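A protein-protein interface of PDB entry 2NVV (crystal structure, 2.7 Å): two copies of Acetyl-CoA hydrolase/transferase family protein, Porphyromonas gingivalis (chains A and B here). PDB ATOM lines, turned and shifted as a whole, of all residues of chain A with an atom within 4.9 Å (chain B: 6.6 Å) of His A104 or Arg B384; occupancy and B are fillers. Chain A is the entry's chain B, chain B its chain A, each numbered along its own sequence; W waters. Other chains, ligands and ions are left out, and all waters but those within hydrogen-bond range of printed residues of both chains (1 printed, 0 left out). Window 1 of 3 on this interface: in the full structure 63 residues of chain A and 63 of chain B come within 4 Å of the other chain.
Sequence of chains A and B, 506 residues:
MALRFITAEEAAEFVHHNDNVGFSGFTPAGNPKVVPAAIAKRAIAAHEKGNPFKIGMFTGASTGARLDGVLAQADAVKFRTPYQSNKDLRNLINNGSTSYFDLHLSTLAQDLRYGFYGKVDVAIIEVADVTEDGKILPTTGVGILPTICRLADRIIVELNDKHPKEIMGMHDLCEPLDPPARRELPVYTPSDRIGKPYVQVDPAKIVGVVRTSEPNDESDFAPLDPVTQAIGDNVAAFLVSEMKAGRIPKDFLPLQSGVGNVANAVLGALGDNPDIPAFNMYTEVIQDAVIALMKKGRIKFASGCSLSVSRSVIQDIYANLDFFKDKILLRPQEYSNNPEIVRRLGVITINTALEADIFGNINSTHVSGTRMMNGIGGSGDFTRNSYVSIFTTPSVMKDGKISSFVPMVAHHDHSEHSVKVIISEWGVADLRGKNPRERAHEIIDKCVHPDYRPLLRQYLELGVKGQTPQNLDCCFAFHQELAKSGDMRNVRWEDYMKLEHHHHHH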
ATOM      1  N   ASP A 102      -9.587  21.999  13.380  1.00  0.00           N
ATOM      2  CA  ASP A 102      -8.197  21.568  13.354  1.00  0.00           C
ATOM      3  C   ASP A 102      -7.699  21.323  14.771  1.00  0.00           C
ATOM      4  O   ASP A 102      -7.960  22.102  15.690  1.00  0.00           O
ATOM      5  CB  ASP A 102      -7.297  22.590  12.627  1.00  0.00           C
ATOM      6  CG  ASP A 102      -7.544  24.026  13.058  1.00  0.00           C
ATOM      7  OD1 ASP A 102      -6.606  24.852  12.975  1.00  0.00           O
ATOM      8  OD2 ASP A 102      -8.680  24.335  13.458  1.00  0.00           O
ATOM      9  N   LEU A 103      -6.978  20.225  14.939  1.00  0.00           N
ATOM     10  CA  LEU A 103      -6.474  19.831  16.246  1.00  0.00           C
ATOM     11  C   LEU A 103      -4.962  19.668  16.246  1.00  0.00           C
ATOM     12  O   LEU A 103      -4.331  19.631  15.188  1.00  0.00           O
ATOM     13  CB  LEU A 103      -7.098  18.490  16.648  1.00  0.00           C
ATOM     14  CG  LEU A 103      -8.622  18.339  16.562  1.00  0.00           C
ATOM     15  CD1 LEU A 103      -8.980  16.865  16.623  1.00  0.00           C
ATOM     16  CD2 LEU A 103      -9.286  19.123  17.691  1.00  0.00           C
ATOM     17  N   HIS A 104      -4.385  19.595  17.443  1.00  0.00           N
ATOM     18  CA  HIS A 104      -2.960  19.365  17.561  1.00  0.00           C
ATOM     19  C   HIS A 104      -2.880  17.914  17.067  1.00  0.00           C
ATOM     20  O   HIS A 104      -3.519  17.020  17.624  1.00  0.00           O
ATOM     21  CB  HIS A 104      -2.512  19.464  19.025  1.00  0.00           C
ATOM     22  CG  HIS A 104      -2.596  20.851  19.597  1.00  0.00           C
ATOM     23  ND1 HIS A 104      -1.911  21.921  19.062  1.00  0.00           N
ATOM     24  CD2 HIS A 104      -3.280  21.339  20.662  1.00  0.00           C
ATOM     25  CE1 HIS A 104      -2.169  23.008  19.771  1.00  0.00           C
ATOM     26  NE2 HIS A 104      -2.996  22.683  20.747  1.00  0.00           N
ATOM     27  N   LEU A 105      -2.117  17.685  16.007  1.00  0.00           N
ATOM     28  CA  LEU A 105      -2.011  16.354  15.435  1.00  0.00           C
ATOM     29  C   LEU A 105      -1.685  15.204  16.383  1.00  0.00           C
ATOM     30  O   LEU A 105      -2.243  14.121  16.230  1.00  0.00           O
ATOM     31  CB  LEU A 105      -1.007  16.364  14.283  1.00  0.00           C
ATOM     32  CG  LEU A 105      -1.364  17.353  13.168  1.00  0.00           C
ATOM     33  CD1 LEU A 105      -0.429  17.150  11.989  1.00  0.00           C
ATOM     34  CD2 LEU A 105      -2.808  17.150  12.747  1.00  0.00           C
ATOM     35  N   SER A 106      -0.804  15.417  17.354  1.00  0.00           N
ATOM     36  CA  SER A 106      -0.439  14.334  18.269  1.00  0.00           C
ATOM     37  C   SER A 106      -1.573  13.816  19.166  1.00  0.00           C
ATOM     38  O   SER A 106      -1.470  12.725  19.746  1.00  0.00           O
ATOM     39  CB  SER A 106       0.715  14.777  19.165  1.00  0.00           C
ATOM     40  OG  SER A 106       0.262  15.691  20.142  1.00  0.00           O
ATOM     41  N   THR A 107      -2.661  14.580  19.257  1.00  0.00           N
ATOM     42  CA  THR A 107      -3.771  14.221  20.134  1.00  0.00           C
ATOM     43  C   THR A 107      -4.963  13.466  19.560  1.00  0.00           C
ATOM     44  O   THR A 107      -5.732  12.882  20.315  1.00  0.00           O
ATOM     45  CB  THR A 107      -4.327  15.474  20.835  1.00  0.00           C
ATOM     46  OG1 THR A 107      -4.981  16.311  19.872  1.00  0.00           O
ATOM     47  CG2 THR A 107      -3.207  16.257  21.496  1.00  0.00           C
ATOM     48  N   LEU A 108      -5.126  13.456  18.243  1.00  0.00           N
ATOM     49  CA  LEU A 108      -6.280  12.781  17.642  1.00  0.00           C
ATOM     50  C   LEU A 108      -6.427  11.289  17.938  1.00  0.00           C
ATOM     51  O   LEU A 108      -7.529  10.820  18.233  1.00  0.00           O
ATOM     52  CB  LEU A 108      -6.300  13.007  16.124  1.00  0.00           C
ATOM     53  CG  LEU A 108      -7.475  12.377  15.365  1.00  0.00           C
ATOM     54  CD1 LEU A 108      -8.804  12.897  15.899  1.00  0.00           C
ATOM     55  CD2 LEU A 108      -7.349  12.692  13.885  1.00  0.00           C
ATOM     56  N   ILE A 376      -3.768  24.243  12.379  1.00  0.00           N
ATOM     57  CA  ILE A 376      -2.649  24.469  13.280  1.00  0.00           C
ATOM     58  C   ILE A 376      -1.592  23.391  13.068  1.00  0.00           C
ATOM     59  O   ILE A 376      -0.405  23.627  13.302  1.00  0.00           O
ATOM     60  CB  ILE A 376      -3.094  24.473  14.759  1.00  0.00           C
ATOM     61  CG1 ILE A 376      -1.934  24.950  15.640  1.00  0.00           C
ATOM     62  CG2 ILE A 376      -3.557  23.081  15.176  1.00  0.00           C
ATOM     63  CD1 ILE A 376      -2.303  25.208  17.083  1.00  0.00           C
ATOM     64  N   GLY A 377      -2.024  22.219  12.604  1.00  0.00           N
ATOM     65  CA  GLY A 377      -1.110  21.118  12.360  1.00  0.00           C
ATOM     66  C   GLY A 377      -0.396  20.657  13.618  1.00  0.00           C
ATOM     67  O   GLY A 377      -1.000  20.548  14.680  1.00  0.00           O
ATOM     68  N   GLY A 380       1.894  23.347  17.072  1.00  0.00           N
ATOM     69  CA  GLY A 380       1.675  23.512  18.496  1.00  0.00           C
ATOM     70  C   GLY A 380       2.391  22.418  19.270  1.00  0.00           C
ATOM     71  O   GLY A 380       3.095  22.702  20.234  1.00  0.00           O
ATOM     72  N   ASP A 381       2.212  21.167  18.847  1.00  0.00           N
ATOM     73  CA  ASP A 381       2.867  20.031  19.498  1.00  0.00           C
ATOM     74  C   ASP A 381       4.370  20.269  19.617  1.00  0.00           C
ATOM     75  O   ASP A 381       4.978  19.990  20.650  1.00  0.00           O
ATOM     76  CB  ASP A 381       2.655  18.739  18.691  1.00  0.00           C
ATOM     77  CG  ASP A 381       1.211  18.289  18.661  1.00  0.00           C
ATOM     78  OD1 ASP A 381       0.595  18.147  19.743  1.00  0.00           O
ATOM     79  OD2 ASP A 381       0.700  18.061  17.544  1.00  0.00           O
ATOM     80  N   ARG A 384       5.505  24.357  21.330  1.00  0.00           N
ATOM     81  CA  ARG A 384       5.286  24.335  22.765  1.00  0.00           C
ATOM     82  C   ARG A 384       6.332  23.568  23.553  1.00  0.00           C
ATOM     83  O   ARG A 384       6.761  24.032  24.605  1.00  0.00           O
ATOM     84  CB  ARG A 384       3.904  23.759  23.083  1.00  0.00           C
ATOM     85  CG  ARG A 384       3.649  23.557  24.576  1.00  0.00           C
ATOM     86  CD  ARG A 384       3.636  24.878  25.351  1.00  0.00           C
ATOM     87  NE  ARG A 384       2.353  25.578  25.252  1.00  0.00           N
ATOM     88  CZ  ARG A 384       1.287  25.294  26.000  1.00  0.00           C
ATOM     89  NH1 ARG A 384       0.159  25.974  25.846  1.00  0.00           N
ATOM     90  NH2 ARG A 384       1.351  24.333  26.916  1.00  0.00           N
ATOM     91  N   VAL B 342       1.583  14.720  33.039  1.00  0.00           N
ATOM     92  CA  VAL B 342       0.198  15.146  32.934  1.00  0.00           C
ATOM     93  C   VAL B 342      -0.564  14.340  31.880  1.00  0.00           C
ATOM     94  O   VAL B 342      -1.620  13.770  32.159  1.00  0.00           O
ATOM     95  CB  VAL B 342       0.122  16.656  32.597  1.00  0.00           C
ATOM     96  CG1 VAL B 342      -1.310  17.088  32.384  1.00  0.00           C
ATOM     97  CG2 VAL B 342       0.726  17.468  33.727  1.00  0.00           C
ATOM     98  N   ARG B 343      -0.014  14.288  30.670  1.00  0.00           N
ATOM     99  CA  ARG B 343      -0.645  13.557  29.577  1.00  0.00           C
ATOM    100  C   ARG B 343      -0.652  12.043  29.773  1.00  0.00           C
ATOM    101  O   ARG B 343      -1.621  11.376  29.431  1.00  0.00           O
ATOM    102  CB  ARG B 343       0.037  13.910  28.256  1.00  0.00           C
ATOM    103  CG  ARG B 343      -0.608  13.266  27.041  1.00  0.00           C
ATOM    104  CD  ARG B 343      -0.369  14.074  25.781  1.00  0.00           C
ATOM    105  NE  ARG B 343      -0.522  13.244  24.597  1.00  0.00           N
ATOM    106  CZ  ARG B 343      -0.470  13.693  23.350  1.00  0.00           C
ATOM    107  NH1 ARG B 343      -0.280  14.984  23.109  1.00  0.00           N
ATOM    108  NH2 ARG B 343      -0.563  12.835  22.336  1.00  0.00           N
ATOM    109  N   THR B 349      -7.754  18.603  34.154  1.00  0.00           N
ATOM    110  CA  THR B 349      -7.413  19.934  34.640  1.00  0.00           C
ATOM    111  C   THR B 349      -8.586  20.901  34.674  1.00  0.00           C
ATOM    112  O   THR B 349      -9.380  20.960  33.736  1.00  0.00           O
ATOM    113  CB  THR B 349      -6.269  20.556  33.793  1.00  0.00           C
ATOM    114  OG1 THR B 349      -6.714  20.756  32.456  1.00  0.00           O
ATOM    115  CG2 THR B 349      -5.064  19.640  33.760  1.00  0.00           C
ATOM    116  N   SER B 379      -1.271  26.949  34.070  1.00  0.00           N
ATOM    117  CA  SER B 379      -2.515  26.685  33.352  1.00  0.00           C
ATOM    118  C   SER B 379      -2.244  26.163  31.951  1.00  0.00           C
ATOM    119  O   SER B 379      -3.024  25.380  31.425  1.00  0.00           O
ATOM    120  CB  SER B 379      -3.383  27.942  33.279  1.00  0.00           C
ATOM    121  OG  SER B 379      -2.725  28.978  32.594  1.00  0.00           O
ATOM    122  N   GLY B 380      -1.141  26.603  31.350  1.00  0.00           N
ATOM    123  CA  GLY B 380      -0.779  26.135  30.027  1.00  0.00           C
ATOM    124  C   GLY B 380      -0.225  24.715  30.095  1.00  0.00           C
ATOM    125  O   GLY B 380      -0.629  23.854  29.311  1.00  0.00           O
ATOM    126  N   ASP B 381       0.701  24.459  31.022  1.00  0.00           N
ATOM    127  CA  ASP B 381       1.284  23.121  31.181  1.00  0.00           C
ATOM    128  C   ASP B 381       0.179  22.075  31.322  1.00  0.00           C
ATOM    129  O   ASP B 381       0.235  21.011  30.717  1.00  0.00           O
ATOM    130  CB  ASP B 381       2.174  23.047  32.433  1.00  0.00           C
ATOM    131  CG  ASP B 381       3.423  23.914  32.335  1.00  0.00           C
ATOM    132  OD1 ASP B 381       4.183  23.794  31.354  1.00  0.00           O
ATOM    133  OD2 ASP B 381       3.661  24.715  33.260  1.00  0.00           O
ATOM    134  N   PHE B 382      -0.821  22.392  32.136  1.00  0.00           N
ATOM    135  CA  PHE B 382      -1.930  21.497  32.385  1.00  0.00           C
ATOM    136  C   PHE B 382      -2.968  21.453  31.259  1.00  0.00           C
ATOM    137  O   PHE B 382      -3.141  20.426  30.601  1.00  0.00           O
ATOM    138  CB  PHE B 382      -2.580  21.891  33.701  1.00  0.00           C
ATOM    139  CG  PHE B 382      -1.765  21.514  34.903  1.00  0.00           C
ATOM    140  CD1 PHE B 382      -1.676  20.191  35.314  1.00  0.00           C
ATOM    141  CD2 PHE B 382      -1.060  22.480  35.611  1.00  0.00           C
ATOM    142  CE1 PHE B 382      -0.904  19.840  36.405  1.00  0.00           C
ATOM    143  CE2 PHE B 382      -0.282  22.130  36.704  1.00  0.00           C
ATOM    144  CZ  PHE B 382      -0.207  20.807  37.099  1.00  0.00           C
ATOM    145  N   THR B 383      -3.654  22.567  31.040  1.00  0.00           N
ATOM    146  CA  THR B 383      -4.676  22.661  29.992  1.00  0.00           C
ATOM    147  C   THR B 383      -4.276  21.966  28.691  1.00  0.00           C
ATOM    148  O   THR B 383      -5.004  21.112  28.178  1.00  0.00           O
ATOM    149  CB  THR B 383      -4.989  24.129  29.640  1.00  0.00           C
ATOM    150  OG1 THR B 383      -5.481  24.806  30.799  1.00  0.00           O
ATOM    151  CG2 THR B 383      -6.018  24.199  28.545  1.00  0.00           C
ATOM    152  N   ARG B 384      -3.115  22.350  28.169  1.00  0.00           N
ATOM    153  CA  ARG B 384      -2.610  21.801  26.923  1.00  0.00           C
ATOM    154  C   ARG B 384      -2.505  20.279  26.881  1.00  0.00           C
ATOM    155  O   ARG B 384      -2.837  19.667  25.863  1.00  0.00           O
ATOM    156  CB  ARG B 384      -1.249  22.416  26.593  1.00  0.00           C
ATOM    157  CG  ARG B 384      -0.564  21.786  25.385  1.00  0.00           C
ATOM    158  CD  ARG B 384      -1.338  22.029  24.105  1.00  0.00           C
ATOM    159  NE  ARG B 384      -1.044  23.348  23.540  1.00  0.00           N
ATOM    160  CZ  ARG B 384       0.026  23.626  22.795  1.00  0.00           C
ATOM    161  NH1 ARG B 384       0.216  24.853  22.323  1.00  0.00           N
ATOM    162  NH2 ARG B 384       0.898  22.670  22.504  1.00  0.00           N
ATOM    163  N   ASN B 385      -2.073  19.662  27.979  1.00  0.00           N
ATOM    164  CA  ASN B 385      -1.897  18.211  27.999  1.00  0.00           C
ATOM    165  C   ASN B 385      -2.886  17.361  28.789  1.00  0.00           C
ATOM    166  O   ASN B 385      -2.754  16.142  28.825  1.00  0.00           O
ATOM    167  CB  ASN B 385      -0.484  17.886  28.469  1.00  0.00           C
ATOM    168  CG  ASN B 385       0.577  18.632  27.673  1.00  0.00           C
ATOM    169  OD1 ASN B 385       1.158  19.615  28.149  1.00  0.00           O
ATOM    170  ND2 ASN B 385       0.820  18.181  26.449  1.00  0.00           N
ATOM    171  N   SER B 386      -3.888  17.987  29.400  1.00  0.00           N
ATOM    172  CA  SER B 386      -4.867  17.243  30.180  1.00  0.00           C
ATOM    173  C   SER B 386      -5.747  16.319  29.347  1.00  0.00           C
ATOM    174  O   SER B 386      -5.911  16.508  28.140  1.00  0.00           O
ATOM    175  CB  SER B 386      -5.778  18.189  30.947  1.00  0.00           C
ATOM    176  OG  SER B 386      -6.572  18.922  30.038  1.00  0.00           O
ATOM    177  N   SER B 389      -9.547  19.404  29.292  1.00  0.00           N
ATOM    178  CA  SER B 389      -9.262  20.658  29.982  1.00  0.00           C
ATOM    179  C   SER B 389     -10.545  21.432  30.223  1.00  0.00           C
ATOM    180  O   SER B 389     -11.360  21.593  29.319  1.00  0.00           O
ATOM    181  CB  SER B 389      -8.290  21.517  29.178  1.00  0.00           C
ATOM    182  OG  SER B 389      -8.904  21.969  27.988  1.00  0.00           O
ATOM    183  N   HIS B 414      -4.783  30.830  26.205  1.00  0.00           N
ATOM    184  CA  HIS B 414      -5.096  29.464  25.775  1.00  0.00           C
ATOM    185  C   HIS B 414      -5.957  29.545  24.524  1.00  0.00           C
ATOM    186  O   HIS B 414      -6.872  30.352  24.461  1.00  0.00           O
ATOM    187  CB  HIS B 414      -5.807  28.714  26.900  1.00  0.00           C
ATOM    188  CG  HIS B 414      -5.083  28.792  28.208  1.00  0.00           C
ATOM    189  ND1 HIS B 414      -5.285  29.817  29.109  1.00  0.00           N
ATOM    190  CD2 HIS B 414      -4.088  28.032  28.720  1.00  0.00           C
ATOM    191  CE1 HIS B 414      -4.445  29.686  30.120  1.00  0.00           C
ATOM    192  NE2 HIS B 414      -3.707  28.611  29.908  1.00  0.00           N
ATOM    193  N   SER B 415      -5.654  28.719  23.527  1.00  0.00           N
ATOM    194  CA  SER B 415      -6.384  28.748  22.272  1.00  0.00           C
ATOM    195  C   SER B 415      -7.493  27.707  22.109  1.00  0.00           C
ATOM    196  O   SER B 415      -7.584  26.731  22.869  1.00  0.00           O
ATOM    197  CB  SER B 415      -5.419  28.599  21.102  1.00  0.00           C
ATOM    198  OG  SER B 415      -5.126  27.237  20.872  1.00  0.00           O
ATOM    199  N   HIS B 417      -7.749  25.396  20.293  1.00  0.00           N
ATOM    200  CA  HIS B 417      -7.209  24.052  20.110  1.00  0.00           C
ATOM    201  C   HIS B 417      -6.862  23.369  21.422  1.00  0.00           C
ATOM    202  O   HIS B 417      -6.602  22.172  21.449  1.00  0.00           O
ATOM    203  CB  HIS B 417      -5.946  24.112  19.248  1.00  0.00           C
ATOM    204  CG  HIS B 417      -6.125  24.881  17.979  1.00  0.00           C
ATOM    205  ND1 HIS B 417      -6.900  24.423  16.935  1.00  0.00           N
ATOM    206  CD2 HIS B 417      -5.681  26.105  17.609  1.00  0.00           C
ATOM    207  CE1 HIS B 417      -6.932  25.332  15.978  1.00  0.00           C
ATOM    208  NE2 HIS B 417      -6.199  26.362  16.363  1.00  0.00           N
ATOM    209  N   SER B 418      -6.864  24.129  22.508  1.00  0.00           N
ATOM    210  CA  SER B 418      -6.504  23.573  23.798  1.00  0.00           C
ATOM    211  C   SER B 418      -7.633  23.554  24.808  1.00  0.00           C
ATOM    212  O   SER B 418      -7.658  22.700  25.685  1.00  0.00           O
ATOM    213  CB  SER B 418      -5.314  24.349  24.376  1.00  0.00           C
ATOM    214  OG  SER B 418      -4.165  24.223  23.557  1.00  0.00           O
ATOM    215  N   LYS B 420     -11.065  22.609  26.020  1.00  0.00           N
ATOM    216  CA  LYS B 420     -12.081  21.606  25.701  1.00  0.00           C
ATOM    217  C   LYS B 420     -13.461  21.845  26.297  1.00  0.00           C
ATOM    218  O   LYS B 420     -14.476  21.539  25.663  1.00  0.00           O
ATOM    219  CB  LYS B 420     -11.596  20.223  26.132  1.00  0.00           C
ATOM    220  CG  LYS B 420     -10.204  19.869  25.622  1.00  0.00           C
ATOM    221  CD  LYS B 420     -10.103  20.016  24.119  1.00  0.00           C
ATOM    222  CE  LYS B 420      -8.699  19.703  23.620  1.00  0.00           C
ATOM    223  NZ  LYS B 420      -8.631  19.813  22.141  1.00  0.00           N
HETATM  224  O   HOH W   1      -2.199  26.949  23.747  1.00  0.00           O
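The guanidinium group (NH2) of Arg B384 sits at hydrogen-bond distance from the backbone carbonyl oxygen (O) of Gly A380 (3.2 Å). The side-chain hydroxyl (OG) of Ser B418 lies within hydrogen-bond range of a ring nitrogen (NE2) of His A104 (3.4 Å). The guanidinium group of Arg A384 lies within hydrogen-bond range of the backbone carbonyl oxygen of Gly B380, at 3.1 Å. The backbone carbonyl oxygen of Asp A102 lies within hydrogen-bond range of a ring nitrogen (ND1) of His B417. NE2 of His A104 lies within hydrogen-bond range of NE of Arg B384 (3.5 Å). The guanidinium group (NH2) of Arg B343 is in hydrogen-bond range of the backbone carbonyl oxygen (O) of Ser A106 (2.7 Å).
The side-chain amino group (NZ) of Lys B420 is in hydrogen-bond range of the backbone carbonyl oxygen (O) of His B417 (3.2 Å). OG of Ser B389 lies within hydrogen-bond range of O of Ser B418, 2.7 Å away. The backbone carbonyl oxygen of His A104 lies within hydrogen-bond range of the side-chain hydroxyl of Thr A107. The side-chain hydroxyl of Ser A106 is in hydrogen-bond range of the side-chain carboxylate of Asp A381 (2.5 Å). OG of Ser B415 lies close to N of His B417, at 3.3 Å. The guanidinium group (NE) of Arg B384 is in hydrogen-bond range of the side-chain hydroxyl (OG) of Ser B418, 3.2 Å away.
Among the printed residues, merely in contact across the chains: Arg A384 with Arg B384, His A104 with His B417, Ile A376 with His B417 and Thr A107 with Arg B343.
His A104 touches just these residues of chain B: Arg B384 (3.5 Å), His B417 (3.5 Å) and Ser B418 (3.4 Å). Arg B384 touches three residues of chain A. Printed residues of chain B within 4 Å of Arg A384: Gly B380 (3.1 Å) and Arg B384 (3.2 Å). Of the printed residues of chain A, Ser B418 touches His A104. Of the printed residues of chain B, Ile A376 touches His B417 (3.5 Å). Lys B420 touches none of the printed residues of chain A. Ser B389 touches none of the printed residues of chain A.
Printed residues of chain A that touch a printed residue of chain B: Asp A102, His A104, Ser A106, Thr A107, Ile A376, Gly A380 and Arg A384. Hydrophobic or aromatic side chains of chain A within 4 Å of the printed part of chain B: His A104 and Ile A376. Along chain B the printed residues that touch a printed residue of chain A span positions 343 to 418. Among the printed residues, 10 pairs touch across the chains. Among the printed residues, no Asp or Glu carboxylate lies within 4 Å of a Lys or Arg side-chain nitrogen of the other chain.
Gly A380 touches Arg B384, and with the chains exchanged Arg A384 touches Gly B380. Arg A384 touches its own counterpart, Arg B384. 3 positions are printed for both chains.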
